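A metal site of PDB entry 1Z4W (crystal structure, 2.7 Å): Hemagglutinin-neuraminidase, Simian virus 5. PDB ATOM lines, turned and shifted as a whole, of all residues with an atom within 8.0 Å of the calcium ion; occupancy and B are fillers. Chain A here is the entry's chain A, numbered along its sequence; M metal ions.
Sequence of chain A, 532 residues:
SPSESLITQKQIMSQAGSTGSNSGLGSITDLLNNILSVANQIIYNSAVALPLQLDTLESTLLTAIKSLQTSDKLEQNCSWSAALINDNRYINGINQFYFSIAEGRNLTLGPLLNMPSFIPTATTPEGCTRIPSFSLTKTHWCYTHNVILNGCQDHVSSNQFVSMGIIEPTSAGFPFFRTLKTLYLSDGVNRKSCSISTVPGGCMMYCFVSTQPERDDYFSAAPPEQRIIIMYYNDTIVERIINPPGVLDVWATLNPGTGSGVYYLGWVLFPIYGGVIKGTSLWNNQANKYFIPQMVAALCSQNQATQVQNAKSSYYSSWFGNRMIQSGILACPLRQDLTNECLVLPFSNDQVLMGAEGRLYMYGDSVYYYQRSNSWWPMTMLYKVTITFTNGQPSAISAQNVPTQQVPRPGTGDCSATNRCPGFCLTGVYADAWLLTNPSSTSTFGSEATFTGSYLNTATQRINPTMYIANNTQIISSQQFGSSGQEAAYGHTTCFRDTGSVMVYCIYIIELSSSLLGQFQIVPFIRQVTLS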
ATOM      1  N   GLN A 212     -27.612   8.443  30.161  1.00  0.00           N
ATOM      2  CA  GLN A 212     -26.538   7.793  30.888  1.00  0.00           C
ATOM      3  C   GLN A 212     -25.315   8.680  30.846  1.00  0.00           C
ATOM      4  O   GLN A 212     -25.254   9.623  30.057  1.00  0.00           O
ATOM      5  CB  GLN A 212     -26.221   6.454  30.239  1.00  0.00           C
ATOM      6  CG  GLN A 212     -25.691   6.579  28.826  1.00  0.00           C
ATOM      7  CD  GLN A 212     -25.596   5.241  28.130  1.00  0.00           C
ATOM      8  OE1 GLN A 212     -25.486   4.203  28.787  1.00  0.00           O
ATOM      9  NE2 GLN A 212     -25.608   5.249  26.801  1.00  0.00           N
ATOM     10  N   GLU A 214     -21.837  10.411  30.014  1.00  0.00           N
ATOM     11  CA  GLU A 214     -21.223  10.609  28.717  1.00  0.00           C
ATOM     12  C   GLU A 214     -20.346   9.448  28.294  1.00  0.00           C
ATOM     13  O   GLU A 214     -20.453   8.944  27.181  1.00  0.00           O
ATOM     14  CB  GLU A 214     -20.396  11.904  28.718  1.00  0.00           C
ATOM     15  CG  GLU A 214     -19.507  12.045  27.484  1.00  0.00           C
ATOM     16  CD  GLU A 214     -18.861  13.403  27.371  1.00  0.00           C
ATOM     17  OE1 GLU A 214     -18.350  13.907  28.392  1.00  0.00           O
ATOM     18  OE2 GLU A 214     -18.863  13.971  26.249  1.00  0.00           O
ATOM     19  N   ARG A 215     -19.460   9.028  29.189  1.00  0.00           N
ATOM     20  CA  ARG A 215     -18.557   7.942  28.869  1.00  0.00           C
ATOM     21  C   ARG A 215     -19.278   6.684  28.412  1.00  0.00           C
ATOM     22  O   ARG A 215     -18.824   5.990  27.496  1.00  0.00           O
ATOM     23  CB  ARG A 215     -17.683   7.632  30.064  1.00  0.00           C
ATOM     24  CG  ARG A 215     -16.520   6.745  29.718  1.00  0.00           C
ATOM     25  CD  ARG A 215     -15.717   6.426  30.940  1.00  0.00           C
ATOM     26  NE  ARG A 215     -14.671   5.469  30.624  1.00  0.00           N
ATOM     27  CZ  ARG A 215     -14.113   4.668  31.521  1.00  0.00           C
ATOM     28  NH1 ARG A 215     -14.518   4.712  32.788  1.00  0.00           N
ATOM     29  NH2 ARG A 215     -13.171   3.817  31.158  1.00  0.00           N
ATOM     30  N   ASP A 216     -20.409   6.373  29.033  1.00  0.00           N
ATOM     31  CA  ASP A 216     -21.160   5.184  28.664  1.00  0.00           C
ATOM     32  C   ASP A 216     -21.654   5.295  27.226  1.00  0.00           C
ATOM     33  O   ASP A 216     -21.762   4.296  26.519  1.00  0.00           O
ATOM     34  CB  ASP A 216     -22.339   4.978  29.620  1.00  0.00           C
ATOM     35  CG  ASP A 216     -21.893   4.817  31.062  1.00  0.00           C
ATOM     36  OD1 ASP A 216     -20.666   4.834  31.294  1.00  0.00           O
ATOM     37  OD2 ASP A 216     -22.758   4.673  31.947  1.00  0.00           O
ATOM     38  N   ASP A 217     -21.959   6.511  26.784  1.00  0.00           N
ATOM     39  CA  ASP A 217     -22.418   6.696  25.412  1.00  0.00           C
ATOM     40  C   ASP A 217     -21.348   6.223  24.427  1.00  0.00           C
ATOM     41  O   ASP A 217     -21.655   5.664  23.398  1.00  0.00           O
ATOM     42  CB  ASP A 217     -22.741   8.159  25.111  1.00  0.00           C
ATOM     43  CG  ASP A 217     -24.048   8.601  25.710  1.00  0.00           C
ATOM     44  OD1 ASP A 217     -25.013   7.810  25.668  1.00  0.00           O
ATOM     45  OD2 ASP A 217     -24.126   9.745  26.212  1.00  0.00           O
ATOM     46  N   TYR A 218     -20.081   6.445  24.754  1.00  0.00           N
ATOM     47  CA  TYR A 218     -19.027   6.012  23.857  1.00  0.00           C
ATOM     48  C   TYR A 218     -18.837   4.497  23.808  1.00  0.00           C
ATOM     49  O   TYR A 218     -18.483   3.936  22.771  1.00  0.00           O
ATOM     50  CB  TYR A 218     -17.712   6.691  24.224  1.00  0.00           C
ATOM     51  CG  TYR A 218     -17.666   8.149  23.823  1.00  0.00           C
ATOM     52  CD1 TYR A 218     -18.227   9.135  24.644  1.00  0.00           C
ATOM     53  CD2 TYR A 218     -17.139   8.546  22.591  1.00  0.00           C
ATOM     54  CE1 TYR A 218     -18.272  10.462  24.245  1.00  0.00           C
ATOM     55  CE2 TYR A 218     -17.177   9.875  22.185  1.00  0.00           C
ATOM     56  CZ  TYR A 218     -17.747  10.828  23.014  1.00  0.00           C
ATOM     57  OH  TYR A 218     -17.806  12.152  22.614  1.00  0.00           O
ATOM     58  N   PHE A 219     -19.096   3.819  24.932  1.00  0.00           N
ATOM     59  CA  PHE A 219     -18.963   2.369  24.971  1.00  0.00           C
ATOM     60  C   PHE A 219     -20.150   1.658  24.334  1.00  0.00           C
ATOM     61  O   PHE A 219     -19.974   0.627  23.682  1.00  0.00           O
ATOM     62  CB  PHE A 219     -18.798   1.886  26.412  1.00  0.00           C
ATOM     63  CG  PHE A 219     -17.414   2.076  26.933  1.00  0.00           C
ATOM     64  CD1 PHE A 219     -17.024   3.283  27.493  1.00  0.00           C
ATOM     65  CD2 PHE A 219     -16.477   1.052  26.836  1.00  0.00           C
ATOM     66  CE1 PHE A 219     -15.718   3.476  27.936  1.00  0.00           C
ATOM     67  CE2 PHE A 219     -15.170   1.238  27.263  1.00  0.00           C
ATOM     68  CZ  PHE A 219     -14.788   2.454  27.818  1.00  0.00           C
ATOM     69  N   SER A 220     -21.360   2.181  24.500  1.00  0.00           N
ATOM     70  CA  SER A 220     -22.527   1.551  23.888  1.00  0.00           C
ATOM     71  C   SER A 220     -22.396   1.708  22.379  1.00  0.00           C
ATOM     72  O   SER A 220     -22.019   2.771  21.873  1.00  0.00           O
ATOM     73  CB  SER A 220     -23.825   2.203  24.388  1.00  0.00           C
ATOM     74  OG  SER A 220     -23.887   3.573  24.063  1.00  0.00           O
ATOM     75  N   ALA A 221     -22.671   0.645  21.639  1.00  0.00           N
ATOM     76  CA  ALA A 221     -22.556   0.682  20.184  1.00  0.00           C
ATOM     77  C   ALA A 221     -23.677   1.497  19.566  1.00  0.00           C
ATOM     78  O   ALA A 221     -23.531   2.045  18.467  1.00  0.00           O
ATOM     79  CB  ALA A 221     -22.572  -0.737  19.624  1.00  0.00           C
ATOM     80  N   ALA A 222     -24.808   1.590  20.246  1.00  0.00           N
ATOM     81  CA  ALA A 222     -25.950   2.344  19.745  1.00  0.00           C
ATOM     82  C   ALA A 222     -25.787   3.807  20.131  1.00  0.00           C
ATOM     83  O   ALA A 222     -25.427   4.095  21.252  1.00  0.00           O
ATOM     84  CB  ALA A 222     -27.232   1.796  20.324  1.00  0.00           C
ATOM     85  N   PRO A 223     -26.072   4.734  19.222  1.00  0.00           N
ATOM     86  CA  PRO A 223     -25.958   6.163  19.486  1.00  0.00           C
ATOM     87  C   PRO A 223     -27.208   6.673  20.200  1.00  0.00           C
ATOM     88  O   PRO A 223     -28.258   6.039  20.135  1.00  0.00           O
ATOM     89  CB  PRO A 223     -25.812   6.745  18.090  1.00  0.00           C
ATOM     90  CG  PRO A 223     -26.738   5.876  17.300  1.00  0.00           C
ATOM     91  CD  PRO A 223     -26.403   4.485  17.805  1.00  0.00           C
ATOM     92  N   PRO A 224     -27.104   7.817  20.902  1.00  0.00           N
ATOM     93  CA  PRO A 224     -28.290   8.334  21.594  1.00  0.00           C
ATOM     94  C   PRO A 224     -29.316   8.796  20.573  1.00  0.00           C
ATOM     95  O   PRO A 224     -29.010   8.895  19.381  1.00  0.00           O
ATOM     96  CB  PRO A 224     -27.741   9.504  22.404  1.00  0.00           C
ATOM     97  CG  PRO A 224     -26.301   9.180  22.567  1.00  0.00           C
ATOM     98  CD  PRO A 224     -25.924   8.614  21.238  1.00  0.00           C
ATOM     99  N   TRP A 251     -21.350   5.557  14.262  1.00  0.00           N
ATOM    100  CA  TRP A 251     -21.039   6.405  15.396  1.00  0.00           C
ATOM    101  C   TRP A 251     -21.564   5.788  16.688  1.00  0.00           C
ATOM    102  O   TRP A 251     -22.740   5.440  16.774  1.00  0.00           O
ATOM    103  CB  TRP A 251     -21.661   7.796  15.221  1.00  0.00           C
ATOM    104  CG  TRP A 251     -21.114   8.598  14.055  1.00  0.00           C
ATOM    105  CD1 TRP A 251     -21.264   8.331  12.726  1.00  0.00           C
ATOM    106  CD2 TRP A 251     -20.353   9.808  14.147  1.00  0.00           C
ATOM    107  NE1 TRP A 251     -20.658   9.313  11.975  1.00  0.00           N
ATOM    108  CE2 TRP A 251     -20.094  10.230  12.817  1.00  0.00           C
ATOM    109  CE3 TRP A 251     -19.871  10.590  15.207  1.00  0.00           C
ATOM    110  CZ2 TRP A 251     -19.366  11.393  12.530  1.00  0.00           C
ATOM    111  CZ3 TRP A 251     -19.157  11.750  14.920  1.00  0.00           C
ATOM    112  CH2 TRP A 251     -18.899  12.140  13.590  1.00  0.00           C
ATOM    113  N   ALA A 252     -20.697   5.624  17.682  1.00  0.00           N
ATOM    114  CA  ALA A 252     -21.133   5.068  18.957  1.00  0.00           C
ATOM    115  C   ALA A 252     -21.926   6.166  19.647  1.00  0.00           C
ATOM    116  O   ALA A 252     -22.822   5.889  20.403  1.00  0.00           O
ATOM    117  CB  ALA A 252     -19.936   4.645  19.797  1.00  0.00           C
ATOM    118  N   THR A 253     -21.588   7.418  19.385  1.00  0.00           N
ATOM    119  CA  THR A 253     -22.287   8.570  19.955  1.00  0.00           C
ATOM    120  C   THR A 253     -22.230   9.687  18.937  1.00  0.00           C
ATOM    121  O   THR A 253     -21.386   9.673  18.040  1.00  0.00           O
ATOM    122  CB  THR A 253     -21.618   9.126  21.202  1.00  0.00           C
ATOM    123  OG1 THR A 253     -20.747   8.142  21.766  1.00  0.00           O
ATOM    124  CG2 THR A 253     -22.668   9.519  22.235  1.00  0.00           C
ATOM    125  N   LEU A 254     -23.110  10.662  19.117  1.00  0.00           N
ATOM    126  CA  LEU A 254     -23.179  11.819  18.240  1.00  0.00           C
ATOM    127  C   LEU A 254     -23.780  12.950  19.079  1.00  0.00           C
ATOM    128  O   LEU A 254     -24.798  12.764  19.747  1.00  0.00           O
ATOM    129  CB  LEU A 254     -24.064  11.505  17.034  1.00  0.00           C
ATOM    130  CG  LEU A 254     -24.270  12.610  15.995  1.00  0.00           C
ATOM    131  CD1 LEU A 254     -22.919  13.124  15.487  1.00  0.00           C
ATOM    132  CD2 LEU A 254     -25.092  12.057  14.845  1.00  0.00           C
ATOM    133  N   GLY A 275     -18.009   9.738  18.701  1.00  0.00           N
ATOM    134  CA  GLY A 275     -17.040   8.664  18.571  1.00  0.00           C
ATOM    135  C   GLY A 275     -17.394   7.685  17.474  1.00  0.00           C
ATOM    136  O   GLY A 275     -18.512   7.194  17.412  1.00  0.00           O
ATOM    137  N   ILE A 277     -16.955   4.096  15.476  1.00  0.00           N
ATOM    138  CA  ILE A 277     -16.631   2.686  15.680  1.00  0.00           C
ATOM    139  C   ILE A 277     -15.520   2.170  14.779  1.00  0.00           C
ATOM    140  O   ILE A 277     -15.476   2.453  13.573  1.00  0.00           O
ATOM    141  CB  ILE A 277     -17.899   1.842  15.486  1.00  0.00           C
ATOM    142  CG1 ILE A 277     -18.917   2.206  16.585  1.00  0.00           C
ATOM    143  CG2 ILE A 277     -17.573   0.362  15.487  1.00  0.00           C
ATOM    144  CD1 ILE A 277     -20.289   1.627  16.378  1.00  0.00           C
ATOM    145  N   ARG A 323     -12.937   4.785  20.706  1.00  0.00           N
ATOM    146  CA  ARG A 323     -13.530   5.299  19.480  1.00  0.00           C
ATOM    147  C   ARG A 323     -12.626   6.366  18.873  1.00  0.00           C
ATOM    148  O   ARG A 323     -11.704   6.872  19.513  1.00  0.00           O
ATOM    149  CB  ARG A 323     -14.879   5.945  19.776  1.00  0.00           C
ATOM    150  CG  ARG A 323     -15.830   5.112  20.607  1.00  0.00           C
ATOM    151  CD  ARG A 323     -16.143   3.813  19.911  1.00  0.00           C
ATOM    152  NE  ARG A 323     -17.168   3.055  20.622  1.00  0.00           N
ATOM    153  CZ  ARG A 323     -17.470   1.794  20.339  1.00  0.00           C
ATOM    154  NH1 ARG A 323     -16.831   1.156  19.368  1.00  0.00           N
ATOM    155  NH2 ARG A 323     -18.418   1.167  21.035  1.00  0.00           N
HETATM  156 CA    CA M   1     -23.537   4.928  22.252  1.00  0.00          CA
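The side-chain hydroxyl (OG) of Ser 220 lies close to the backbone carbonyl oxygen (O) of Asp 216, at 3.3 Å.
O of Asp 217 sits close to OG1 of Thr 253 (3.1 Å).
The backbone NH of Ala 252 sits at hydrogen-bond distance from the backbone carbonyl oxygen of Gly 275, at 2.7 Å.
OD1 of Asp 217 is in hydrogen-bond range of NE2 of Gln 212 (2.9 Å).
Residues that only touch the calcium ion: Pro 223 (3.9 Å).
Five residues have an atom within 4 Å of the calcium ion: Asp 217, Ser 220, Ala 222, Pro 223 and Ala 252.
O of Ala 252 is bound to the calcium ion (2.2 Å).
OG of Ser 220 binds the calcium ion (2.3 Å).
The backbone carbonyl oxygen (O) of Ala 222 is bound to the calcium ion, 2.3 Å away.
The calcium ion is bound by O of Asp 217 (2.3 Å).
The calcium ion is bound by O of Ser 220.
The calcium ion has five donor atoms within binding distance.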
